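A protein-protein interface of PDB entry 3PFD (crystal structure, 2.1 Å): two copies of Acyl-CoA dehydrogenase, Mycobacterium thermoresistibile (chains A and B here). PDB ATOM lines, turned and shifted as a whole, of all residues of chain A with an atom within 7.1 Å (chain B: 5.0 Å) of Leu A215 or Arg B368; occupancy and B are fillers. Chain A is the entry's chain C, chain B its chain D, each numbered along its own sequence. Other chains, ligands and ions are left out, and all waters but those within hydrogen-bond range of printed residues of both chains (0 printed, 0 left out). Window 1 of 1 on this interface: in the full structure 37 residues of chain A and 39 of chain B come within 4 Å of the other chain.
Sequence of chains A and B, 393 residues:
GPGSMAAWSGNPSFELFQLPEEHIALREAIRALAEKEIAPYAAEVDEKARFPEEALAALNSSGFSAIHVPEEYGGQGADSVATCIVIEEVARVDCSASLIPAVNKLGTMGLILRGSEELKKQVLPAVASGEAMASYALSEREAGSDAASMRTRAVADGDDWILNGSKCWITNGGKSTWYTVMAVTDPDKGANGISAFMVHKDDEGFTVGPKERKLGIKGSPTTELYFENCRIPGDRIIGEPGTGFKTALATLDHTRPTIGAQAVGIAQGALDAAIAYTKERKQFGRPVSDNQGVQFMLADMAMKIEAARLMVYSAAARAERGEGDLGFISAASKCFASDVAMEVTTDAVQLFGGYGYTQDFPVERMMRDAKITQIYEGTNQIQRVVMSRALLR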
ATOM      1  N   ASP A  46      -3.437 -23.175   7.066  1.00  0.00           N
ATOM      2  CA  ASP A  46      -3.887 -23.900   8.223  1.00  0.00           C
ATOM      3  C   ASP A  46      -2.751 -24.490   9.050  1.00  0.00           C
ATOM      4  O   ASP A  46      -2.782 -24.415  10.277  1.00  0.00           O
ATOM      5  CB  ASP A  46      -4.819 -25.019   7.771  1.00  0.00           C
ATOM      6  CG  ASP A  46      -5.139 -25.990   8.879  1.00  0.00           C
ATOM      7  OD1 ASP A  46      -5.997 -25.675   9.721  1.00  0.00           O
ATOM      8  OD2 ASP A  46      -4.540 -27.071   8.890  1.00  0.00           O
ATOM      9  N   ARG A 213      -5.680 -19.733  19.719  1.00  0.00           N
ATOM     10  CA  ARG A 213      -5.299 -21.064  19.198  1.00  0.00           C
ATOM     11  C   ARG A 213      -6.591 -21.849  18.934  1.00  0.00           C
ATOM     12  O   ARG A 213      -7.359 -22.077  19.859  1.00  0.00           O
ATOM     13  CB  ARG A 213      -4.454 -21.831  20.215  1.00  0.00           C
ATOM     14  CG  ARG A 213      -3.026 -21.313  20.399  1.00  0.00           C
ATOM     15  CD  ARG A 213      -2.286 -22.049  21.520  1.00  0.00           C
ATOM     16  NE  ARG A 213      -3.074 -22.047  22.765  1.00  0.00           N
ATOM     17  CZ  ARG A 213      -3.359 -23.122  23.518  1.00  0.00           C
ATOM     18  NH1 ARG A 213      -2.921 -24.339  23.185  1.00  0.00           N
ATOM     19  NH2 ARG A 213      -4.092 -22.972  24.619  1.00  0.00           N
ATOM     20  N   LYS A 214      -6.834 -22.251  17.694  1.00  0.00           N
ATOM     21  CA  LYS A 214      -8.200 -22.696  17.313  1.00  0.00           C
ATOM     22  C   LYS A 214      -8.271 -24.089  16.719  1.00  0.00           C
ATOM     23  O   LYS A 214      -7.266 -24.649  16.277  1.00  0.00           O
ATOM     24  CB  LYS A 214      -8.888 -21.693  16.370  1.00  0.00           C
ATOM     25  CG  LYS A 214      -8.908 -20.273  16.869  1.00  0.00           C
ATOM     26  CD  LYS A 214      -9.959 -19.411  16.136  1.00  0.00           C
ATOM     27  CE  LYS A 214      -9.595 -19.124  14.668  1.00  0.00           C
ATOM     28  NZ  LYS A 214      -8.157 -18.740  14.454  1.00  0.00           N
ATOM     29  N   LEU A 215      -9.481 -24.639  16.712  1.00  0.00           N
ATOM     30  CA  LEU A 215      -9.776 -25.908  16.061  1.00  0.00           C
ATOM     31  C   LEU A 215      -9.553 -25.815  14.540  1.00  0.00           C
ATOM     32  O   LEU A 215      -8.922 -26.679  13.934  1.00  0.00           O
ATOM     33  CB  LEU A 215     -11.234 -26.304  16.370  1.00  0.00           C
ATOM     34  CG  LEU A 215     -11.870 -27.446  15.588  1.00  0.00           C
ATOM     35  CD1 LEU A 215     -10.995 -28.686  15.614  1.00  0.00           C
ATOM     36  CD2 LEU A 215     -13.316 -27.754  16.151  1.00  0.00           C
ATOM     37  N   GLY A 216     -10.087 -24.759  13.937  1.00  0.00           N
ATOM     38  CA  GLY A 216     -10.027 -24.581  12.496  1.00  0.00           C
ATOM     39  C   GLY A 216      -9.963 -23.104  12.181  1.00  0.00           C
ATOM     40  O   GLY A 216      -9.644 -22.290  13.059  1.00  0.00           O
ATOM     41  N   ILE A 217     -10.276 -22.747  10.931  1.00  0.00           N
ATOM     42  CA  ILE A 217      -9.898 -21.451  10.348  1.00  0.00           C
ATOM     43  C   ILE A 217      -8.607 -20.933  11.015  1.00  0.00           C
ATOM     44  O   ILE A 217      -8.517 -19.765  11.457  1.00  0.00           O
ATOM     45  CB  ILE A 217     -11.060 -20.402  10.321  1.00  0.00           C
ATOM     46  CG1 ILE A 217     -11.663 -20.207  11.721  1.00  0.00           C
ATOM     47  CG2 ILE A 217     -12.124 -20.854   9.323  1.00  0.00           C
ATOM     48  CD1 ILE A 217     -12.448 -18.932  11.896  1.00  0.00           C
ATOM     49  N   LYS A 218      -7.630 -21.840  11.109  1.00  0.00           N
ATOM     50  CA  LYS A 218      -6.415 -21.584  11.865  1.00  0.00           C
ATOM     51  C   LYS A 218      -5.686 -20.324  11.368  1.00  0.00           C
ATOM     52  O   LYS A 218      -5.156 -19.578  12.167  1.00  0.00           O
ATOM     53  CB  LYS A 218      -5.482 -22.784  11.822  1.00  0.00           C
ATOM     54  CG  LYS A 218      -5.937 -23.953  12.667  1.00  0.00           C
ATOM     55  CD  LYS A 218      -4.774 -24.808  13.032  1.00  0.00           C
ATOM     56  CE  LYS A 218      -5.231 -25.984  13.842  1.00  0.00           C
ATOM     57  NZ  LYS A 218      -4.086 -26.861  14.072  1.00  0.00           N
ATOM     58  N   MET A 342     -21.413 -29.401   8.739  1.00  0.00           N
ATOM     59  CA  MET A 342     -20.858 -30.261   9.790  1.00  0.00           C
ATOM     60  C   MET A 342     -21.041 -31.738   9.467  1.00  0.00           C
ATOM     61  O   MET A 342     -20.109 -32.549   9.620  1.00  0.00           O
ATOM     62  CB  MET A 342     -21.476 -29.926  11.173  1.00  0.00           C
ATOM     63  CG  MET A 342     -20.626 -30.373  12.354  1.00  0.00           C
ATOM     64  SD  MET A 342     -18.965 -29.643  12.396  1.00  0.00           S
ATOM     65  CE  MET A 342     -17.920 -31.034  11.815  1.00  0.00           C
ATOM     66  N   TYR A 357      -8.235 -38.946   7.652  1.00  0.00           N
ATOM     67  CA  TYR A 357      -7.828 -38.559   8.991  1.00  0.00           C
ATOM     68  C   TYR A 357      -6.426 -37.965   8.988  1.00  0.00           C
ATOM     69  O   TYR A 357      -5.906 -37.628  10.049  1.00  0.00           O
ATOM     70  CB  TYR A 357      -7.903 -39.790   9.933  1.00  0.00           C
ATOM     71  CG  TYR A 357      -8.048 -39.461  11.399  1.00  0.00           C
ATOM     72  CD1 TYR A 357      -9.262 -39.006  11.933  1.00  0.00           C
ATOM     73  CD2 TYR A 357      -6.972 -39.602  12.252  1.00  0.00           C
ATOM     74  CE1 TYR A 357      -9.377 -38.696  13.292  1.00  0.00           C
ATOM     75  CE2 TYR A 357      -7.077 -39.308  13.623  1.00  0.00           C
ATOM     76  CZ  TYR A 357      -8.274 -38.860  14.129  1.00  0.00           C
ATOM     77  OH  TYR A 357      -8.351 -38.561  15.467  1.00  0.00           O
ATOM     78  N   GLU A 364     -10.040 -33.309   6.333  1.00  0.00           N
ATOM     79  CA  GLU A 364      -9.736 -33.117   7.746  1.00  0.00           C
ATOM     80  C   GLU A 364      -9.798 -31.588   8.121  1.00  0.00           C
ATOM     81  O   GLU A 364     -10.460 -31.175   9.086  1.00  0.00           O
ATOM     82  CB  GLU A 364      -8.322 -33.720   7.841  1.00  0.00           C
ATOM     83  CG  GLU A 364      -7.540 -33.706   9.019  1.00  0.00           C
ATOM     84  CD  GLU A 364      -6.933 -32.392   9.332  1.00  0.00           C
ATOM     85  OE1 GLU A 364      -6.169 -31.781   8.523  1.00  0.00           O
ATOM     86  OE2 GLU A 364      -7.200 -32.015  10.462  1.00  0.00           O
ATOM     87  N   ARG A 365      -9.124 -30.745   7.344  1.00  0.00           N
ATOM     88  CA  ARG A 365      -9.218 -29.292   7.566  1.00  0.00           C
ATOM     89  C   ARG A 365     -10.642 -28.759   7.365  1.00  0.00           C
ATOM     90  O   ARG A 365     -11.161 -27.964   8.168  1.00  0.00           O
ATOM     91  CB  ARG A 365      -8.236 -28.542   6.661  1.00  0.00           C
ATOM     92  CG  ARG A 365      -8.344 -27.040   6.785  1.00  0.00           C
ATOM     93  CD  ARG A 365      -7.584 -26.344   5.656  1.00  0.00           C
ATOM     94  NE  ARG A 365      -8.255 -26.352   4.350  1.00  0.00           N
ATOM     95  CZ  ARG A 365      -7.769 -26.936   3.247  1.00  0.00           C
ATOM     96  NH1 ARG A 365      -6.640 -27.648   3.281  1.00  0.00           N
ATOM     97  NH2 ARG A 365      -8.436 -26.846   2.101  1.00  0.00           N
ATOM     98  N   MET A 367     -13.410 -30.256   7.865  1.00  0.00           N
ATOM     99  CA  MET A 367     -14.269 -30.674   8.965  1.00  0.00           C
ATOM    100  C   MET A 367     -14.052 -29.724  10.132  1.00  0.00           C
ATOM    101  O   MET A 367     -15.017 -29.211  10.745  1.00  0.00           O
ATOM    102  CB  MET A 367     -13.930 -32.128   9.364  1.00  0.00           C
ATOM    103  CG  MET A 367     -14.845 -32.684  10.442  1.00  0.00           C
ATOM    104  SD  MET A 367     -14.382 -34.349  10.934  1.00  0.00           S
ATOM    105  CE  MET A 367     -15.307 -34.474  12.476  1.00  0.00           C
ATOM    106  N   ARG A 368     -12.771 -29.480  10.432  1.00  0.00           N
ATOM    107  CA  ARG A 368     -12.388 -28.552  11.496  1.00  0.00           C
ATOM    108  C   ARG A 368     -12.949 -27.134  11.253  1.00  0.00           C
ATOM    109  O   ARG A 368     -13.515 -26.531  12.171  1.00  0.00           O
ATOM    110  CB  ARG A 368     -10.871 -28.532  11.682  1.00  0.00           C
ATOM    111  CG  ARG A 368     -10.318 -29.865  12.242  1.00  0.00           C
ATOM    112  CD  ARG A 368      -8.833 -29.761  12.562  1.00  0.00           C
ATOM    113  NE  ARG A 368      -7.977 -29.832  11.381  1.00  0.00           N
ATOM    114  CZ  ARG A 368      -7.314 -28.807  10.840  1.00  0.00           C
ATOM    115  NH1 ARG A 368      -7.455 -27.560  11.331  1.00  0.00           N
ATOM    116  NH2 ARG A 368      -6.542 -29.024   9.773  1.00  0.00           N
ATOM    117  N   ASP A 369     -12.824 -26.642  10.019  1.00  0.00           N
ATOM    118  CA  ASP A 369     -13.392 -25.349   9.615  1.00  0.00           C
ATOM    119  C   ASP A 369     -14.919 -25.323   9.693  1.00  0.00           C
ATOM    120  O   ASP A 369     -15.499 -24.310  10.066  1.00  0.00           O
ATOM    121  CB  ASP A 369     -12.993 -24.996   8.164  1.00  0.00           C
ATOM    122  CG  ASP A 369     -11.485 -24.796   7.987  1.00  0.00           C
ATOM    123  OD1 ASP A 369     -10.729 -24.712   9.015  1.00  0.00           O
ATOM    124  OD2 ASP A 369     -11.064 -24.724   6.800  1.00  0.00           O
ATOM    125  N   LYS A 371     -16.995 -26.570  11.641  1.00  0.00           N
ATOM    126  CA  LYS A 371     -17.492 -26.404  13.004  1.00  0.00           C
ATOM    127  C   LYS A 371     -17.733 -24.949  13.412  1.00  0.00           C
ATOM    128  O   LYS A 371     -18.681 -24.682  14.137  1.00  0.00           O
ATOM    129  CB  LYS A 371     -16.567 -27.081  14.034  1.00  0.00           C
ATOM    130  CG  LYS A 371     -17.059 -26.948  15.503  1.00  0.00           C
ATOM    131  CD  LYS A 371     -18.365 -27.770  15.746  1.00  0.00           C
ATOM    132  CE  LYS A 371     -19.267 -27.094  16.812  1.00  0.00           C
ATOM    133  NZ  LYS A 371     -20.630 -27.706  16.785  1.00  0.00           N
ATOM    134  N   ILE A 372     -16.886 -24.017  12.957  1.00  0.00           N
ATOM    135  CA  ILE A 372     -17.063 -22.606  13.326  1.00  0.00           C
ATOM    136  C   ILE A 372     -18.366 -22.023  12.788  1.00  0.00           C
ATOM    137  O   ILE A 372     -18.920 -21.107  13.398  1.00  0.00           O
ATOM    138  CB  ILE A 372     -15.852 -21.678  12.914  1.00  0.00           C
ATOM    139  CG1 ILE A 372     -15.933 -20.300  13.589  1.00  0.00           C
ATOM    140  CG2 ILE A 372     -15.818 -21.469  11.406  1.00  0.00           C
ATOM    141  CD1 ILE A 372     -15.953 -20.324  15.157  1.00  0.00           C
ATOM    142  N   ILE A 375     -21.221 -21.669  15.016  1.00  0.00           N
ATOM    143  CA  ILE A 375     -20.918 -20.911  16.243  1.00  0.00           C
ATOM    144  C   ILE A 375     -20.934 -19.409  16.028  1.00  0.00           C
ATOM    145  O   ILE A 375     -21.627 -18.707  16.771  1.00  0.00           O
ATOM    146  CB  ILE A 375     -19.580 -21.350  16.921  1.00  0.00           C
ATOM    147  CG1 ILE A 375     -19.618 -22.828  17.284  1.00  0.00           C
ATOM    148  CG2 ILE A 375     -19.226 -20.451  18.176  1.00  0.00           C
ATOM    149  CD1 ILE A 375     -18.305 -23.362  17.776  1.00  0.00           C
ATOM    150  N   ASP B  46      -1.277 -33.800  22.614  1.00  0.00           N
ATOM    151  CA  ASP B  46      -1.970 -33.429  21.372  1.00  0.00           C
ATOM    152  C   ASP B  46      -1.329 -32.242  20.667  1.00  0.00           C
ATOM    153  O   ASP B  46      -1.019 -32.330  19.471  1.00  0.00           O
ATOM    154  CB  ASP B  46      -3.469 -33.115  21.625  1.00  0.00           C
ATOM    155  CG  ASP B  46      -4.130 -32.450  20.434  1.00  0.00           C
ATOM    156  OD1 ASP B  46      -4.500 -33.168  19.479  1.00  0.00           O
ATOM    157  OD2 ASP B  46      -4.257 -31.204  20.423  1.00  0.00           O
ATOM    158  N   LEU B 215      -5.621 -35.680  12.132  1.00  0.00           N
ATOM    159  CA  LEU B 215      -6.678 -34.865  12.674  1.00  0.00           C
ATOM    160  C   LEU B 215      -6.649 -34.824  14.214  1.00  0.00           C
ATOM    161  O   LEU B 215      -6.765 -33.760  14.824  1.00  0.00           O
ATOM    162  CB  LEU B 215      -8.031 -35.388  12.164  1.00  0.00           C
ATOM    163  CG  LEU B 215      -9.327 -34.844  12.766  1.00  0.00           C
ATOM    164  CD1 LEU B 215      -9.343 -33.329  12.794  1.00  0.00           C
ATOM    165  CD2 LEU B 215     -10.534 -35.376  11.973  1.00  0.00           C
ATOM    166  N   GLY B 216      -6.476 -35.994  14.821  1.00  0.00           N
ATOM    167  CA  GLY B 216      -6.531 -36.182  16.262  1.00  0.00           C
ATOM    168  C   GLY B 216      -5.677 -37.399  16.595  1.00  0.00           C
ATOM    169  O   GLY B 216      -4.856 -37.831  15.774  1.00  0.00           O
ATOM    170  N   LYS B 218      -3.144 -37.135  18.002  1.00  0.00           N
ATOM    171  CA  LYS B 218      -1.879 -36.624  17.447  1.00  0.00           C
ATOM    172  C   LYS B 218      -0.634 -37.171  18.122  1.00  0.00           C
ATOM    173  O   LYS B 218       0.400 -37.380  17.450  1.00  0.00           O
ATOM    174  CB  LYS B 218      -1.855 -35.095  17.502  1.00  0.00           C
ATOM    175  CG  LYS B 218      -2.779 -34.415  16.501  1.00  0.00           C
ATOM    176  CD  LYS B 218      -2.645 -32.891  16.588  1.00  0.00           C
ATOM    177  CE  LYS B 218      -3.348 -32.225  15.436  1.00  0.00           C
ATOM    178  NZ  LYS B 218      -3.149 -30.756  15.409  1.00  0.00           N
ATOM    179  N   VAL B 349     -18.395 -29.237  21.942  1.00  0.00           N
ATOM    180  CA  VAL B 349     -17.737 -28.027  21.395  1.00  0.00           C
ATOM    181  C   VAL B 349     -18.804 -26.909  21.280  1.00  0.00           C
ATOM    182  O   VAL B 349     -18.585 -25.794  21.753  1.00  0.00           O
ATOM    183  CB  VAL B 349     -17.052 -28.288  20.016  1.00  0.00           C
ATOM    184  CG1 VAL B 349     -16.574 -26.990  19.354  1.00  0.00           C
ATOM    185  CG2 VAL B 349     -15.835 -29.258  20.167  1.00  0.00           C
ATOM    186  N   TYR B 357     -14.269 -23.803  20.565  1.00  0.00           N
ATOM    187  CA  TYR B 357     -13.452 -23.759  19.340  1.00  0.00           C
ATOM    188  C   TYR B 357     -11.947 -23.477  19.597  1.00  0.00           C
ATOM    189  O   TYR B 357     -11.153 -23.446  18.661  1.00  0.00           O
ATOM    190  CB  TYR B 357     -14.028 -22.736  18.349  1.00  0.00           C
ATOM    191  CG  TYR B 357     -13.734 -23.029  16.891  1.00  0.00           C
ATOM    192  CD1 TYR B 357     -14.356 -24.099  16.230  1.00  0.00           C
ATOM    193  CD2 TYR B 357     -12.875 -22.207  16.156  1.00  0.00           C
ATOM    194  CE1 TYR B 357     -14.093 -24.356  14.912  1.00  0.00           C
ATOM    195  CE2 TYR B 357     -12.604 -22.465  14.818  1.00  0.00           C
ATOM    196  CZ  TYR B 357     -13.220 -23.547  14.211  1.00  0.00           C
ATOM    197  OH  TYR B 357     -12.969 -23.841  12.904  1.00  0.00           O
ATOM    198  N   THR B 358     -11.560 -23.289  20.859  1.00  0.00           N
ATOM    199  CA  THR B 358     -10.169 -22.971  21.177  1.00  0.00           C
ATOM    200  C   THR B 358      -9.453 -24.133  21.842  1.00  0.00           C
ATOM    201  O   THR B 358     -10.093 -24.967  22.459  1.00  0.00           O
ATOM    202  CB  THR B 358     -10.024 -21.727  22.098  1.00  0.00           C
ATOM    203  OG1 THR B 358     -10.477 -22.037  23.426  1.00  0.00           O
ATOM    204  CG2 THR B 358     -10.789 -20.552  21.541  1.00  0.00           C
ATOM    205  N   GLU B 364     -12.580 -29.542  21.905  1.00  0.00           N
ATOM    206  CA  GLU B 364     -12.044 -29.475  20.544  1.00  0.00           C
ATOM    207  C   GLU B 364     -11.138 -30.713  20.205  1.00  0.00           C
ATOM    208  O   GLU B 364     -11.322 -31.380  19.191  1.00  0.00           O
ATOM    209  CB  GLU B 364     -11.292 -28.139  20.511  1.00  0.00           C
ATOM    210  CG  GLU B 364     -10.584 -27.772  19.349  1.00  0.00           C
ATOM    211  CD  GLU B 364      -9.169 -28.308  19.285  1.00  0.00           C
ATOM    212  OE1 GLU B 364      -8.407 -28.346  20.286  1.00  0.00           O
ATOM    213  OE2 GLU B 364      -8.848 -28.666  18.157  1.00  0.00           O
ATOM    214  N   ARG B 365     -10.203 -31.034  21.082  1.00  0.00           N
ATOM    215  CA  ARG B 365      -9.364 -32.258  20.949  1.00  0.00           C
ATOM    216  C   ARG B 365     -10.196 -33.529  21.046  1.00  0.00           C
ATOM    217  O   ARG B 365     -10.018 -34.428  20.255  1.00  0.00           O
ATOM    218  CB  ARG B 365      -8.263 -32.279  22.029  1.00  0.00           C
ATOM    219  CG  ARG B 365      -7.358 -33.518  21.995  1.00  0.00           C
ATOM    220  CD  ARG B 365      -6.558 -33.657  23.279  1.00  0.00           C
ATOM    221  NE  ARG B 365      -7.294 -34.227  24.416  1.00  0.00           N
ATOM    222  CZ  ARG B 365      -7.499 -33.617  25.590  1.00  0.00           C
ATOM    223  NH1 ARG B 365      -7.093 -32.354  25.805  1.00  0.00           N
ATOM    224  NH2 ARG B 365      -8.134 -34.277  26.563  1.00  0.00           N
ATOM    225  N   MET B 366     -11.129 -33.585  21.998  1.00  0.00           N
ATOM    226  CA  MET B 366     -12.060 -34.726  22.110  1.00  0.00           C
ATOM    227  C   MET B 366     -12.852 -34.950  20.815  1.00  0.00           C
ATOM    228  O   MET B 366     -13.085 -36.108  20.376  1.00  0.00           O
ATOM    229  CB  MET B 366     -13.042 -34.496  23.280  1.00  0.00           C
ATOM    230  CG  MET B 366     -12.387 -34.565  24.680  1.00  0.00           C
ATOM    231  SD  MET B 366     -13.513 -33.818  25.879  1.00  0.00           S
ATOM    232  CE  MET B 366     -12.564 -34.043  27.395  1.00  0.00           C
ATOM    233  N   MET B 367     -13.283 -33.852  20.202  1.00  0.00           N
ATOM    234  CA  MET B 367     -13.995 -33.918  18.920  1.00  0.00           C
ATOM    235  C   MET B 367     -13.130 -34.504  17.816  1.00  0.00           C
ATOM    236  O   MET B 367     -13.583 -35.363  17.031  1.00  0.00           O
ATOM    237  CB  MET B 367     -14.507 -32.542  18.483  1.00  0.00           C
ATOM    238  CG  MET B 367     -15.332 -32.604  17.191  1.00  0.00           C
ATOM    239  SD  MET B 367     -15.993 -30.993  16.673  1.00  0.00           S
ATOM    240  CE  MET B 367     -16.621 -31.441  15.039  1.00  0.00           C
ATOM    241  N   ARG B 368     -11.875 -34.055  17.765  1.00  0.00           N
ATOM    242  CA  ARG B 368     -10.942 -34.525  16.758  1.00  0.00           C
ATOM    243  C   ARG B 368     -10.616 -36.003  16.998  1.00  0.00           C
ATOM    244  O   ARG B 368     -10.518 -36.777  16.060  1.00  0.00           O
ATOM    245  CB  ARG B 368      -9.671 -33.643  16.756  1.00  0.00           C
ATOM    246  CG  ARG B 368      -9.941 -32.229  16.204  1.00  0.00           C
ATOM    247  CD  ARG B 368      -8.673 -31.383  16.032  1.00  0.00           C
ATOM    248  NE  ARG B 368      -8.222 -30.857  17.320  1.00  0.00           N
ATOM    249  CZ  ARG B 368      -7.186 -31.331  18.007  1.00  0.00           C
ATOM    250  NH1 ARG B 368      -6.463 -32.358  17.542  1.00  0.00           N
ATOM    251  NH2 ARG B 368      -6.871 -30.779  19.170  1.00  0.00           N
ATOM    252  N   ASP B 369     -10.475 -36.391  18.256  1.00  0.00           N
ATOM    253  CA  ASP B 369     -10.167 -37.773  18.611  1.00  0.00           C
ATOM    254  C   ASP B 369     -11.351 -38.718  18.275  1.00  0.00           C
ATOM    255  O   ASP B 369     -11.153 -39.830  17.785  1.00  0.00           O
ATOM    256  CB  ASP B 369      -9.821 -37.877  20.112  1.00  0.00           C
ATOM    257  CG  ASP B 369      -8.464 -37.215  20.476  1.00  0.00           C
ATOM    258  OD1 ASP B 369      -7.686 -36.828  19.575  1.00  0.00           O
ATOM    259  OD2 ASP B 369      -8.169 -37.067  21.687  1.00  0.00           O
ATOM    260  N   ALA B 370     -12.568 -38.292  18.583  1.00  0.00           N
ATOM    261  CA  ALA B 370     -13.764 -39.117  18.362  1.00  0.00           C
ATOM    262  C   ALA B 370     -13.819 -39.654  16.928  1.00  0.00           C
ATOM    263  O   ALA B 370     -14.196 -40.801  16.710  1.00  0.00           O
ATOM    264  CB  ALA B 370     -15.046 -38.302  18.663  1.00  0.00           C
ATOM    265  N   LYS B 371     -13.464 -38.797  15.968  1.00  0.00           N
ATOM    266  CA  LYS B 371     -13.510 -39.156  14.554  1.00  0.00           C
ATOM    267  C   LYS B 371     -12.760 -40.442  14.209  1.00  0.00           C
ATOM    268  O   LYS B 371     -13.221 -41.188  13.378  1.00  0.00           O
ATOM    269  CB  LYS B 371     -13.023 -38.010  13.669  1.00  0.00           C
ATOM    270  CG  LYS B 371     -13.148 -38.320  12.218  1.00  0.00           C
ATOM    271  CD  LYS B 371     -14.615 -38.445  11.808  1.00  0.00           C
ATOM    272  CE  LYS B 371     -14.760 -39.419  10.664  1.00  0.00           C
ATOM    273  NZ  LYS B 371     -16.173 -39.814  10.438  1.00  0.00           N
ATOM    274  N   ILE B 372     -11.619 -40.701  14.848  1.00  0.00           N
ATOM    275  CA  ILE B 372     -10.877 -41.945  14.526  1.00  0.00           C
ATOM    276  C   ILE B 372     -11.687 -43.209  14.903  1.00  0.00           C
ATOM    277  O   ILE B 372     -11.544 -44.256  14.267  1.00  0.00           O
ATOM    278  CB  ILE B 372      -9.422 -42.017  15.146  1.00  0.00           C
ATOM    279  CG1 ILE B 372      -8.586 -43.122  14.458  1.00  0.00           C
ATOM    280  CG2 ILE B 372      -9.486 -42.320  16.660  1.00  0.00           C
ATOM    281  CD1 ILE B 372      -8.481 -42.930  12.889  1.00  0.00           C
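Printed residues of chain B that touch a printed residue of chain A: Leu B215, Gly B216, Val B349, Tyr B357, Thr B358, Glu B364, Met B367, Arg B368, Asp B369, Lys B371 and Ile B372.
Hydrophobic or aromatic side chains of chain B that line the printed part of chain A: Leu B215, Val B349, Tyr B357, Met B367 and Ile B372.
Along chain B the printed residues that touch a printed residue of chain A span positions 215 to 372.
Hydrophobic or aromatic side chains of chain A within 4 Å of the printed part of chain B: Leu A215, Ile A217, Met A342, Tyr A357 and Ile A372.
Among the printed residues, 22 pairs touch across the chains.
The backbone carbonyl oxygen (O) of Arg B368 sits at hydrogen-bond distance from the side-chain hydroxyl (OH) of Tyr A357 (2.9 Å).
The backbone NH (N) of Gly A216 lies close to the side-chain hydroxyl (OH) of Tyr B357, at 3.2 Å.
N of Leu A215 lies within hydrogen-bond range of O of Tyr B357.
The backbone NH of Gly B216 sits close to the side-chain hydroxyl of Tyr A357.
N of Leu B215 sits at hydrogen-bond distance from O of Tyr A357, 2.9 Å away.
The side-chain hydroxyl (OH) of Tyr B357 lies within hydrogen-bond range of the backbone carbonyl oxygen (O) of Arg A368, 2.8 Å away.
Of the printed residues of chain B, Arg A213 touches Thr B358.
Of chain B, only Tyr B357 (2.8 Å), Glu B364 (3.3 Å) and Arg B368 (3.6 Å) come within 4 Å of Leu A215.
Of the printed residues of chain B, Gly A216 touches Tyr B357 (3.1 Å).
Lys A218 touches none of the printed residues of chain B.
Printed residues of chain A within 4 Å of Tyr B357: Lys A214, Leu A215, Gly A216, Ile A217, Arg A368, Asp A369, Lys A371 and Ile A372.
Printed residues of chain A within 4 Å of Met B367: Met A342 (3.5 Å).
Arg B368 touches just these residues of chain A: Leu A215 (3.6 Å), Tyr A357 (2.9 Å) and Arg A368 (3.8 Å).
Ala B370 touches none of the printed residues of chain A.
Of the printed residues of chain A, Lys B371 touches Tyr A357.
The nearest residue of chain B that does not touch Leu A215 is Met B367 (4.2 Å).
Among the printed residues, pairs that only touch across the chains: Arg A213 with Thr B358, Lys A214 with Tyr B357, Leu A215 with Glu B364, Leu A215 with Arg B368, Ile A217 with Tyr B357, Met A342 with Met B367, Tyr A357 with Asp B369, Tyr A357 with Lys B371, Tyr A357 with Ile B372, Glu A364 with Leu B215, Arg A368 with Leu B215, Arg A368 with Arg B368, Asp A369 with Tyr B357, Lys A371 with Val B349, Lys A371 with Tyr B357 and Ile A372 with Tyr B357.
The guanidinium group (NE) of Arg B368 is in salt-bridge range of the side-chain carboxylate (OE2) of Glu B364 (2.4 Å).
OD1 of Asp A46 lies within salt-bridge range of NH1 of Arg A368, 2.9 Å away.
N of Lys A371 sits close to SD of Met A342 (3.7 Å).
The backbone carbonyl oxygen (O) of Leu A215 lies within hydrogen-bond range of the guanidinium group (NH1) of Arg A368 (3.1 Å).
The side-chain amino group of Lys A214 lies within hydrogen-bond range of the backbone carbonyl oxygen of Ile A217 (3.2 Å).
The backbone NH (N) of Ile A217 is in hydrogen-bond range of the side-chain carboxylate (OD1) of Asp A369, 2.8 Å away.
Gly A216 touches Tyr B357, and with the chains exchanged Tyr A357 touches Gly B216.
Tyr A357 touches Asp B369, and with the chains exchanged Asp A369 touches Tyr B357.
Tyr A357 touches Lys B371, and with the chains exchanged Lys A371 touches Tyr B357.
Arg A368 touches its own counterpart, Arg B368.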
